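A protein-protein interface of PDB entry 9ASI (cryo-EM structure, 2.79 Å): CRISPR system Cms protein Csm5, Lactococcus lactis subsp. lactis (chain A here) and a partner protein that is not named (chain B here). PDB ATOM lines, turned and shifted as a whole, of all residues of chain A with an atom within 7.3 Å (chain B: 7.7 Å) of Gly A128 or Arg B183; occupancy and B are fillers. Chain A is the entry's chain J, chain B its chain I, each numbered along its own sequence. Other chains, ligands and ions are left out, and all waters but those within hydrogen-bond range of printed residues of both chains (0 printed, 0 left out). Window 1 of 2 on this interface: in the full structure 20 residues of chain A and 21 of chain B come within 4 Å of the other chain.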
ATOM      1  N   TYR A 125     -31.099  15.121   4.178  1.00  0.00           N
ATOM      2  CA  TYR A 125     -29.867  14.879   3.439  1.00  0.00           C
ATOM      3  C   TYR A 125     -30.221  14.250   2.102  1.00  0.00           C
ATOM      4  O   TYR A 125     -31.303  13.687   1.930  1.00  0.00           O
ATOM      5  CB  TYR A 125     -28.909  13.972   4.214  1.00  0.00           C
ATOM      6  CG  TYR A 125     -29.275  12.508   4.158  1.00  0.00           C
ATOM      7  CD1 TYR A 125     -30.415  12.034   4.789  1.00  0.00           C
ATOM      8  CD2 TYR A 125     -28.483  11.601   3.475  1.00  0.00           C
ATOM      9  CE1 TYR A 125     -30.752  10.699   4.739  1.00  0.00           C
ATOM     10  CE2 TYR A 125     -28.812  10.265   3.422  1.00  0.00           C
ATOM     11  CZ  TYR A 125     -29.949   9.819   4.054  1.00  0.00           C
ATOM     12  OH  TYR A 125     -30.281   8.486   4.002  1.00  0.00           O
ATOM     13  N   ILE A 126     -29.291  14.347   1.156  1.00  0.00           N
ATOM     14  CA  ILE A 126     -29.445  13.740  -0.162  1.00  0.00           C
ATOM     15  C   ILE A 126     -28.600  12.468  -0.185  1.00  0.00           C
ATOM     16  O   ILE A 126     -27.362  12.560  -0.128  1.00  0.00           O
ATOM     17  CB  ILE A 126     -29.036  14.703  -1.283  1.00  0.00           C
ATOM     18  CG1 ILE A 126     -29.929  15.944  -1.252  1.00  0.00           C
ATOM     19  CG2 ILE A 126     -29.121  14.010  -2.633  1.00  0.00           C
ATOM     20  CD1 ILE A 126     -29.827  16.801  -2.481  1.00  0.00           C
ATOM     21  N   PRO A 127     -29.205  11.287  -0.280  1.00  0.00           N
ATOM     22  CA  PRO A 127     -28.453  10.045  -0.065  1.00  0.00           C
ATOM     23  C   PRO A 127     -27.447   9.747  -1.158  1.00  0.00           C
ATOM     24  O   PRO A 127     -27.367  10.454  -2.166  1.00  0.00           O
ATOM     25  CB  PRO A 127     -29.547   8.968  -0.024  1.00  0.00           C
ATOM     26  CG  PRO A 127     -30.851   9.696  -0.004  1.00  0.00           C
ATOM     27  CD  PRO A 127     -30.612  11.031  -0.612  1.00  0.00           C
ATOM     28  N   GLY A 128     -26.659   8.699  -0.950  1.00  0.00           N
ATOM     29  CA  GLY A 128     -25.851   8.173  -2.023  1.00  0.00           C
ATOM     30  C   GLY A 128     -26.697   7.486  -3.076  1.00  0.00           C
ATOM     31  O   GLY A 128     -27.840   7.086  -2.841  1.00  0.00           O
ATOM     32  N   SER A 129     -26.113   7.382  -4.269  1.00  0.00           N
ATOM     33  CA  SER A 129     -26.733   6.860  -5.484  1.00  0.00           C
ATOM     34  C   SER A 129     -27.762   7.830  -6.053  1.00  0.00           C
ATOM     35  O   SER A 129     -28.046   7.795  -7.253  1.00  0.00           O
ATOM     36  CB  SER A 129     -27.389   5.499  -5.236  1.00  0.00           C
ATOM     37  OG  SER A 129     -28.486   5.613  -4.346  1.00  0.00           O
ATOM     38  N   SER A 130     -28.192   8.806  -5.257  1.00  0.00           N
ATOM     39  CA  SER A 130     -28.963   9.903  -5.822  1.00  0.00           C
ATOM     40  C   SER A 130     -28.036  10.871  -6.536  1.00  0.00           C
ATOM     41  O   SER A 130     -28.272  11.241  -7.693  1.00  0.00           O
ATOM     42  CB  SER A 130     -29.754  10.615  -4.726  1.00  0.00           C
ATOM     43  OG  SER A 130     -30.693   9.742  -4.127  1.00  0.00           O
ATOM     44  N   LEU A 131     -26.951  11.260  -5.865  1.00  0.00           N
ATOM     45  CA  LEU A 131     -25.894  11.998  -6.537  1.00  0.00           C
ATOM     46  C   LEU A 131     -25.238  11.164  -7.622  1.00  0.00           C
ATOM     47  O   LEU A 131     -24.716  11.732  -8.580  1.00  0.00           O
ATOM     48  CB  LEU A 131     -24.856  12.474  -5.522  1.00  0.00           C
ATOM     49  CG  LEU A 131     -25.408  13.419  -4.451  1.00  0.00           C
ATOM     50  CD1 LEU A 131     -24.320  13.915  -3.497  1.00  0.00           C
ATOM     51  CD2 LEU A 131     -26.101  14.583  -5.123  1.00  0.00           C
ATOM     52  N   LYS A 132     -25.284   9.834  -7.521  1.00  0.00           N
ATOM     53  CA  LYS A 132     -24.735   9.004  -8.591  1.00  0.00           C
ATOM     54  C   LYS A 132     -25.620   9.038  -9.832  1.00  0.00           C
ATOM     55  O   LYS A 132     -25.113   9.093 -10.953  1.00  0.00           O
ATOM     56  CB  LYS A 132     -24.539   7.568  -8.115  1.00  0.00           C
ATOM     57  CG  LYS A 132     -23.872   6.683  -9.147  1.00  0.00           C
ATOM     58  CD  LYS A 132     -23.611   5.291  -8.613  1.00  0.00           C
ATOM     59  CE  LYS A 132     -22.323   5.227  -7.823  1.00  0.00           C
ATOM     60  NZ  LYS A 132     -21.861   3.822  -7.691  1.00  0.00           N
ATOM     61  N   GLY A 133     -26.943   9.015  -9.658  1.00  0.00           N
ATOM     62  CA  GLY A 133     -27.825   9.237 -10.794  1.00  0.00           C
ATOM     63  C   GLY A 133     -27.680  10.630 -11.380  1.00  0.00           C
ATOM     64  O   GLY A 133     -27.702  10.810 -12.603  1.00  0.00           O
ATOM     65  N   ARG A 136     -24.557  10.658 -13.237  1.00  0.00           N
ATOM     66  CA  ARG A 136     -24.729   9.867 -14.449  1.00  0.00           C
ATOM     67  C   ARG A 136     -25.364  10.704 -15.549  1.00  0.00           C
ATOM     68  O   ARG A 136     -24.857  10.757 -16.676  1.00  0.00           O
ATOM     69  CB  ARG A 136     -25.574   8.629 -14.151  1.00  0.00           C
ATOM     70  CG  ARG A 136     -25.769   7.704 -15.337  1.00  0.00           C
ATOM     71  CD  ARG A 136     -26.637   6.517 -14.965  1.00  0.00           C
ATOM     72  NE  ARG A 136     -26.309   5.997 -13.643  1.00  0.00           N
ATOM     73  CZ  ARG A 136     -25.833   4.781 -13.411  1.00  0.00           C
ATOM     74  NH1 ARG A 136     -25.603   3.929 -14.397  1.00  0.00           N
ATOM     75  NH2 ARG A 136     -25.585   4.409 -12.160  1.00  0.00           N
ATOM     76  N   PHE A 153     -18.238   5.686 -12.044  1.00  0.00           N
ATOM     77  CA  PHE A 153     -18.948   5.602 -10.774  1.00  0.00           C
ATOM     78  C   PHE A 153     -18.599   4.356  -9.972  1.00  0.00           C
ATOM     79  O   PHE A 153     -18.473   4.439  -8.748  1.00  0.00           O
ATOM     80  CB  PHE A 153     -20.473   5.668 -10.996  1.00  0.00           C
ATOM     81  CG  PHE A 153     -20.960   4.896 -12.192  1.00  0.00           C
ATOM     82  CD1 PHE A 153     -21.089   3.518 -12.147  1.00  0.00           C
ATOM     83  CD2 PHE A 153     -21.317   5.557 -13.356  1.00  0.00           C
ATOM     84  CE1 PHE A 153     -21.539   2.813 -13.246  1.00  0.00           C
ATOM     85  CE2 PHE A 153     -21.770   4.859 -14.459  1.00  0.00           C
ATOM     86  CZ  PHE A 153     -21.883   3.484 -14.403  1.00  0.00           C
ATOM     87  N   LEU A 156     -15.585   5.361  -8.621  1.00  0.00           N
ATOM     88  CA  LEU A 156     -15.847   6.538  -7.809  1.00  0.00           C
ATOM     89  C   LEU A 156     -16.511   6.130  -6.500  1.00  0.00           C
ATOM     90  O   LEU A 156     -17.200   5.111  -6.419  1.00  0.00           O
ATOM     91  CB  LEU A 156     -16.741   7.515  -8.577  1.00  0.00           C
ATOM     92  CG  LEU A 156     -17.577   8.581  -7.861  1.00  0.00           C
ATOM     93  CD1 LEU A 156     -16.716   9.728  -7.342  1.00  0.00           C
ATOM     94  CD2 LEU A 156     -18.663   9.089  -8.791  1.00  0.00           C
ATOM     95  N   GLN A 157     -16.293   6.934  -5.463  1.00  0.00           N
ATOM     96  CA  GLN A 157     -16.920   6.717  -4.163  1.00  0.00           C
ATOM     97  C   GLN A 157     -17.709   7.969  -3.800  1.00  0.00           C
ATOM     98  O   GLN A 157     -17.221   8.852  -3.093  1.00  0.00           O
ATOM     99  CB  GLN A 157     -15.870   6.372  -3.100  1.00  0.00           C
ATOM    100  CG  GLN A 157     -15.310   4.963  -3.220  1.00  0.00           C
ATOM    101  CD  GLN A 157     -16.395   3.907  -3.271  1.00  0.00           C
ATOM    102  OE1 GLN A 157     -16.621   3.284  -4.308  1.00  0.00           O
ATOM    103  NE2 GLN A 157     -17.073   3.700  -2.149  1.00  0.00           N
ATOM    104  N   VAL A 158     -18.946   8.041  -4.290  1.00  0.00           N
ATOM    105  CA  VAL A 158     -19.843   9.112  -3.879  1.00  0.00           C
ATOM    106  C   VAL A 158     -20.370   8.807  -2.483  1.00  0.00           C
ATOM    107  O   VAL A 158     -20.644   7.649  -2.141  1.00  0.00           O
ATOM    108  CB  VAL A 158     -20.984   9.289  -4.898  1.00  0.00           C
ATOM    109  CG1 VAL A 158     -21.767   8.003  -5.061  1.00  0.00           C
ATOM    110  CG2 VAL A 158     -21.901  10.429  -4.487  1.00  0.00           C
ATOM    111  N   SER A 159     -20.478   9.843  -1.656  1.00  0.00           N
ATOM    112  CA  SER A 159     -20.931   9.724  -0.280  1.00  0.00           C
ATOM    113  C   SER A 159     -22.297  10.384  -0.127  1.00  0.00           C
ATOM    114  O   SER A 159     -22.837  10.978  -1.063  1.00  0.00           O
ATOM    115  CB  SER A 159     -19.910  10.346   0.672  1.00  0.00           C
ATOM    116  OG  SER A 159     -20.066  11.751   0.738  1.00  0.00           O
ATOM    117  N   ASP A 160     -22.859  10.269   1.073  1.00  0.00           N
ATOM    118  CA  ASP A 160     -24.101  10.958   1.376  1.00  0.00           C
ATOM    119  C   ASP A 160     -23.860  12.461   1.471  1.00  0.00           C
ATOM    120  O   ASP A 160     -22.723  12.939   1.509  1.00  0.00           O
ATOM    121  CB  ASP A 160     -24.700  10.450   2.688  1.00  0.00           C
ATOM    122  CG  ASP A 160     -25.458   9.149   2.527  1.00  0.00           C
ATOM    123  OD1 ASP A 160     -25.790   8.783   1.382  1.00  0.00           O
ATOM    124  OD2 ASP A 160     -25.734   8.495   3.551  1.00  0.00           O
ATOM    125  N   SER A 161     -24.953  13.213   1.499  1.00  0.00           N
ATOM    126  CA  SER A 161     -24.861  14.619   1.847  1.00  0.00           C
ATOM    127  C   SER A 161     -24.653  14.767   3.352  1.00  0.00           C
ATOM    128  O   SER A 161     -24.971  13.873   4.141  1.00  0.00           O
ATOM    129  CB  SER A 161     -26.119  15.371   1.416  1.00  0.00           C
ATOM    130  OG  SER A 161     -26.117  15.613   0.023  1.00  0.00           O
ATOM    131  N   THR B  13     -21.836   7.973   7.701  1.00  0.00           N
ATOM    132  CA  THR B  13     -23.072   7.644   7.014  1.00  0.00           C
ATOM    133  C   THR B  13     -23.437   6.204   7.344  1.00  0.00           C
ATOM    134  O   THR B  13     -22.576   5.392   7.694  1.00  0.00           O
ATOM    135  CB  THR B  13     -22.949   7.819   5.497  1.00  0.00           C
ATOM    136  OG1 THR B  13     -22.160   6.754   4.957  1.00  0.00           O
ATOM    137  CG2 THR B  13     -22.296   9.148   5.167  1.00  0.00           C
ATOM    138  N   GLY B  14     -24.725   5.896   7.238  1.00  0.00           N
ATOM    139  CA  GLY B  14     -25.222   4.595   7.635  1.00  0.00           C
ATOM    140  C   GLY B  14     -24.534   3.440   6.940  1.00  0.00           C
ATOM    141  O   GLY B  14     -24.437   3.410   5.711  1.00  0.00           O
ATOM    142  N   LYS B 118     -34.050   2.698   4.503  1.00  0.00           N
ATOM    143  CA  LYS B 118     -33.974   3.711   3.460  1.00  0.00           C
ATOM    144  C   LYS B 118     -34.611   3.186   2.182  1.00  0.00           C
ATOM    145  O   LYS B 118     -34.349   2.053   1.769  1.00  0.00           O
ATOM    146  CB  LYS B 118     -32.523   4.125   3.198  1.00  0.00           C
ATOM    147  CG  LYS B 118     -31.581   2.975   2.905  1.00  0.00           C
ATOM    148  CD  LYS B 118     -30.277   3.468   2.308  1.00  0.00           C
ATOM    149  CE  LYS B 118     -30.515   4.509   1.231  1.00  0.00           C
ATOM    150  NZ  LYS B 118     -29.241   4.934   0.594  1.00  0.00           N
ATOM    151  N   GLU B 120     -34.690   4.152  -1.726  1.00  0.00           N
ATOM    152  CA  GLU B 120     -33.997   5.042  -2.650  1.00  0.00           C
ATOM    153  C   GLU B 120     -34.634   5.059  -4.033  1.00  0.00           C
ATOM    154  O   GLU B 120     -35.406   5.979  -4.317  1.00  0.00           O
ATOM    155  CB  GLU B 120     -32.525   4.638  -2.724  1.00  0.00           C
ATOM    156  CG  GLU B 120     -31.656   5.611  -3.476  1.00  0.00           C
ATOM    157  CD  GLU B 120     -31.348   5.136  -4.870  1.00  0.00           C
ATOM    158  OE1 GLU B 120     -31.612   3.955  -5.172  1.00  0.00           O
ATOM    159  OE2 GLU B 120     -30.814   5.937  -5.656  1.00  0.00           O
ATOM    160  N   ASN B 121     -34.400   4.035  -4.874  1.00  0.00           N
ATOM    161  CA  ASN B 121     -35.113   3.840  -6.141  1.00  0.00           C
ATOM    162  C   ASN B 121     -34.446   2.728  -6.953  1.00  0.00           C
ATOM    163  O   ASN B 121     -33.411   2.196  -6.539  1.00  0.00           O
ATOM    164  CB  ASN B 121     -35.165   5.134  -6.951  1.00  0.00           C
ATOM    165  CG  ASN B 121     -36.258   5.135  -7.970  1.00  0.00           C
ATOM    166  OD1 ASN B 121     -36.903   4.119  -8.200  1.00  0.00           O
ATOM    167  ND2 ASN B 121     -36.536   6.306  -8.526  1.00  0.00           N
ATOM    168  N   ARG B 133     -36.296  -1.044  -3.488  1.00  0.00           N
ATOM    169  CA  ARG B 133     -35.741  -1.952  -2.501  1.00  0.00           C
ATOM    170  C   ARG B 133     -35.708  -1.264  -1.144  1.00  0.00           C
ATOM    171  O   ARG B 133     -35.933  -0.058  -1.024  1.00  0.00           O
ATOM    172  CB  ARG B 133     -34.340  -2.423  -2.901  1.00  0.00           C
ATOM    173  CG  ARG B 133     -33.237  -1.449  -2.577  1.00  0.00           C
ATOM    174  CD  ARG B 133     -31.953  -1.839  -3.265  1.00  0.00           C
ATOM    175  NE  ARG B 133     -31.880  -1.294  -4.612  1.00  0.00           N
ATOM    176  CZ  ARG B 133     -31.074  -0.308  -4.977  1.00  0.00           C
ATOM    177  NH1 ARG B 133     -30.240   0.253  -4.122  1.00  0.00           N
ATOM    178  NH2 ARG B 133     -31.098   0.116  -6.236  1.00  0.00           N
ATOM    179  N   ARG B 137     -29.938   0.108   7.299  1.00  0.00           N
ATOM    180  CA  ARG B 137     -28.612   0.648   7.534  1.00  0.00           C
ATOM    181  C   ARG B 137     -28.479   1.011   9.001  1.00  0.00           C
ATOM    182  O   ARG B 137     -29.401   1.577   9.593  1.00  0.00           O
ATOM    183  CB  ARG B 137     -28.356   1.876   6.656  1.00  0.00           C
ATOM    184  CG  ARG B 137     -28.034   1.542   5.213  1.00  0.00           C
ATOM    185  CD  ARG B 137     -27.437   2.732   4.495  1.00  0.00           C
ATOM    186  NE  ARG B 137     -28.108   3.973   4.858  1.00  0.00           N
ATOM    187  CZ  ARG B 137     -27.596   5.182   4.680  1.00  0.00           C
ATOM    188  NH1 ARG B 137     -26.396   5.353   4.151  1.00  0.00           N
ATOM    189  NH2 ARG B 137     -28.307   6.246   5.038  1.00  0.00           N
ATOM    190  N   TYR B 176     -15.088   2.977   2.894  1.00  0.00           N
ATOM    191  CA  TYR B 176     -16.180   2.424   3.675  1.00  0.00           C
ATOM    192  C   TYR B 176     -15.778   1.062   4.233  1.00  0.00           C
ATOM    193  O   TYR B 176     -14.687   0.549   3.967  1.00  0.00           O
ATOM    194  CB  TYR B 176     -17.456   2.340   2.831  1.00  0.00           C
ATOM    195  CG  TYR B 176     -17.403   1.345   1.698  1.00  0.00           C
ATOM    196  CD1 TYR B 176     -16.852   1.686   0.473  1.00  0.00           C
ATOM    197  CD2 TYR B 176     -17.913   0.065   1.854  1.00  0.00           C
ATOM    198  CE1 TYR B 176     -16.806   0.780  -0.563  1.00  0.00           C
ATOM    199  CE2 TYR B 176     -17.871  -0.850   0.824  1.00  0.00           C
ATOM    200  CZ  TYR B 176     -17.318  -0.488  -0.380  1.00  0.00           C
ATOM    201  OH  TYR B 176     -17.276  -1.403  -1.408  1.00  0.00           O
ATOM    202  N   GLY B 179     -20.823  -3.505   2.528  1.00  0.00           N
ATOM    203  CA  GLY B 179     -22.133  -3.284   1.955  1.00  0.00           C
ATOM    204  C   GLY B 179     -22.088  -2.377   0.741  1.00  0.00           C
ATOM    205  O   GLY B 179     -21.085  -2.279   0.034  1.00  0.00           O
ATOM    206  N   HIS B 180     -23.199  -1.676   0.516  1.00  0.00           N
ATOM    207  CA  HIS B 180     -23.385  -0.878  -0.693  1.00  0.00           C
ATOM    208  C   HIS B 180     -22.558   0.405  -0.600  1.00  0.00           C
ATOM    209  O   HIS B 180     -23.067   1.524  -0.634  1.00  0.00           O
ATOM    210  CB  HIS B 180     -24.864  -0.568  -0.884  1.00  0.00           C
ATOM    211  CG  HIS B 180     -25.764  -1.729  -0.596  1.00  0.00           C
ATOM    212  ND1 HIS B 180     -26.247  -1.994   0.666  1.00  0.00           N
ATOM    213  CD2 HIS B 180     -26.259  -2.698  -1.400  1.00  0.00           C
ATOM    214  CE1 HIS B 180     -27.008  -3.072   0.626  1.00  0.00           C
ATOM    215  NE2 HIS B 180     -27.030  -3.520  -0.616  1.00  0.00           N
ATOM    216  N   GLY B 181     -21.243   0.214  -0.488  1.00  0.00           N
ATOM    217  CA  GLY B 181     -20.367   1.322  -0.160  1.00  0.00           C
ATOM    218  C   GLY B 181     -20.125   2.290  -1.291  1.00  0.00           C
ATOM    219  O   GLY B 181     -19.809   3.458  -1.048  1.00  0.00           O
ATOM    220  N   THR B 182     -20.266   1.833  -2.532  1.00  0.00           N
ATOM    221  CA  THR B 182     -20.076   2.717  -3.672  1.00  0.00           C
ATOM    222  C   THR B 182     -21.199   3.739  -3.794  1.00  0.00           C
ATOM    223  O   THR B 182     -21.049   4.721  -4.527  1.00  0.00           O
ATOM    224  CB  THR B 182     -19.963   1.881  -4.950  1.00  0.00           C
ATOM    225  OG1 THR B 182     -19.110   0.759  -4.702  1.00  0.00           O
ATOM    226  CG2 THR B 182     -19.339   2.689  -6.066  1.00  0.00           C
ATOM    227  N   ARG B 183     -22.295   3.553  -3.062  1.00  0.00           N
ATOM    228  CA  ARG B 183     -23.484   4.381  -3.214  1.00  0.00           C
ATOM    229  C   ARG B 183     -23.790   5.177  -1.950  1.00  0.00           C
ATOM    230  O   ARG B 183     -24.938   5.211  -1.499  1.00  0.00           O
ATOM    231  CB  ARG B 183     -24.686   3.514  -3.596  1.00  0.00           C
ATOM    232  CG  ARG B 183     -24.809   3.248  -5.089  1.00  0.00           C
ATOM    233  CD  ARG B 183     -25.239   1.825  -5.369  1.00  0.00           C
ATOM    234  NE  ARG B 183     -24.334   0.852  -4.771  1.00  0.00           N
ATOM    235  CZ  ARG B 183     -24.541  -0.457  -4.774  1.00  0.00           C
ATOM    236  NH1 ARG B 183     -25.623  -0.981  -5.321  1.00  0.00           N
ATOM    237  NH2 ARG B 183     -23.641  -1.258  -4.214  1.00  0.00           N
ATOM    238  N   GLY B 184     -22.773   5.794  -1.356  1.00  0.00           N
ATOM    239  CA  GLY B 184     -22.991   6.725  -0.268  1.00  0.00           C
ATOM    240  C   GLY B 184     -23.169   6.119   1.103  1.00  0.00           C
ATOM    241  O   GLY B 184     -23.599   6.829   2.020  1.00  0.00           O
ATOM    242  N   SER B 185     -22.849   4.843   1.285  1.00  0.00           N
ATOM    243  CA  SER B 185     -23.027   4.176   2.564  1.00  0.00           C
ATOM    244  C   SER B 185     -21.704   3.602   3.044  1.00  0.00           C
ATOM    245  O   SER B 185     -20.810   3.304   2.249  1.00  0.00           O
ATOM    246  CB  SER B 185     -24.067   3.055   2.467  1.00  0.00           C
ATOM    247  OG  SER B 185     -23.471   1.847   2.033  1.00  0.00           O
ATOM    248  N   GLY B 186     -21.580   3.464   4.361  1.00  0.00           N
ATOM    249  CA  GLY B 186     -20.473   2.754   4.961  1.00  0.00           C
ATOM    250  C   GLY B 186     -19.321   3.602   5.448  1.00  0.00           C
ATOM    251  O   GLY B 186     -18.324   3.038   5.912  1.00  0.00           O
ATOM    252  N   ARG B 187     -19.415   4.926   5.359  1.00  0.00           N
ATOM    253  CA  ARG B 187     -18.324   5.777   5.817  1.00  0.00           C
ATOM    254  C   ARG B 187     -18.089   5.571   7.309  1.00  0.00           C
ATOM    255  O   ARG B 187     -19.031   5.603   8.106  1.00  0.00           O
ATOM    256  CB  ARG B 187     -18.638   7.243   5.524  1.00  0.00           C
ATOM    257  CG  ARG B 187     -19.234   7.499   4.149  1.00  0.00           C
ATOM    258  CD  ARG B 187     -18.291   7.104   3.030  1.00  0.00           C
ATOM    259  NE  ARG B 187     -18.950   7.149   1.731  1.00  0.00           N
ATOM    260  CZ  ARG B 187     -19.025   6.125   0.892  1.00  0.00           C
ATOM    261  NH1 ARG B 187     -18.495   4.952   1.185  1.00  0.00           N
ATOM    262  NH2 ARG B 187     -19.646   6.284  -0.272  1.00  0.00           N
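OE2 of Glu B120 lies within hydrogen-bond range of OG of Ser A129, 2.7 Å away. OH of Tyr A125 is in hydrogen-bond range of NH2 of Arg B137, at 3.2 Å. The guanidinium group (NH1) of Arg B137 is in salt-bridge range of the side-chain carboxylate (OD2) of Asp A160. NE2 of Gln A157 lies within hydrogen-bond range of O of Gly B181 (3.0 Å). The side-chain amino group of Lys A132 sits close to the backbone carbonyl oxygen of Thr B182, at 3.4 Å. The backbone carbonyl oxygen (O) of Val A158 sits at hydrogen-bond distance from the backbone NH (N) of Gly B184 (2.9 Å). O of Val A158 lies within hydrogen-bond range of NH2 of Arg B187 (2.5 Å). OD1 of Asp A160 sits close to O of Gly B184 (3.0 Å).
OG1 of Thr B13 sits at hydrogen-bond distance from O of Gly B184. The backbone NH (N) of Gly B186 is in hydrogen-bond range of the side-chain hydroxyl (OG1) of Thr B13, 3.4 Å away. The backbone carbonyl oxygen (O) of Gly B14 is in hydrogen-bond range of the guanidinium group (NH1) of Arg B137 (3.2 Å). The guanidinium group (NH2) of Arg B187 sits at hydrogen-bond distance from the backbone carbonyl oxygen (O) of Gly B181 (2.9 Å). O of Ser B185 sits at hydrogen-bond distance from NH1 of Arg B187. The backbone NH (N) of Gly A128 is in hydrogen-bond range of the side-chain carboxylate (OD1) of Asp A160 (2.5 Å).
Among the printed residues, merely in contact across the chains: Gly A128 with Arg B183 (3.1 Å), Gly A128 with Gly B184 (3.7 Å), Ser A129 with Arg B183 (3.4 Å), Ser A130 with Glu B120 (3.9 Å), Lys A132 with Arg B183 (3.97 Å), Phe A153 with Thr B182 (3.3 Å), Leu A156 with Thr B182 (3.3 Å), Gln A157 with Tyr B176 (3.3 Å), Gln A157 with Thr B182 (3.3 Å), Gln A157 with Arg B187 (3.8 Å), Val A158 with Thr B182 (3.4 Å), Ser A159 with Gly B184 (3.6 Å), Ser A159 with Arg B187 (3.5 Å) and Asp A160 with Thr B13 (3.5 Å).
Gly A128 touches just these residues of chain B: Arg B183 and Gly B184. Printed residues of chain A within 4 Å of Arg B183: Gly A128 (3.1 Å), Ser A129 (3.4 Å) and Lys A132 (3.97 Å). Of the printed residues of chain B, Ser A129 touches Glu B120 (2.7 Å) and Arg B183 (3.4 Å). Of the printed residues of chain B, Ser A130 touches Glu B120. Of the printed residues of chain A, Thr B182 touches Lys A132 (3.2 Å), Phe A153 (3.3 Å), Leu A156 (3.3 Å), Gln A157 (3.3 Å) and Val A158 (3.4 Å). Printed residues of chain B within 4 Å of Ser A159: Gly B184 and Arg B187. Of the printed residues of chain A, Glu B120 touches Ser A129 and Ser A130. Arg A136 touches none of the printed residues of chain B. The nearest residue of chain B that does not touch Gly A128 is Glu B120 (4.1 Å). The nearest printed residue of chain A that does not touch Arg B137 is Pro A127 (5.9 Å).
Of the 17 printed residues of chain B, 9 touch a printed residue of chain A. Printed residues of chain A that touch a printed residue of chain B: Tyr A125, Gly A128, Ser A129, Ser A130, Lys A132, Phe A153, Leu A156, Gln A157, Val A158, Ser A159 and Asp A160. Hydrophobic or aromatic side chains of chain A that line the printed part of chain B: Tyr A125 and Val A158.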
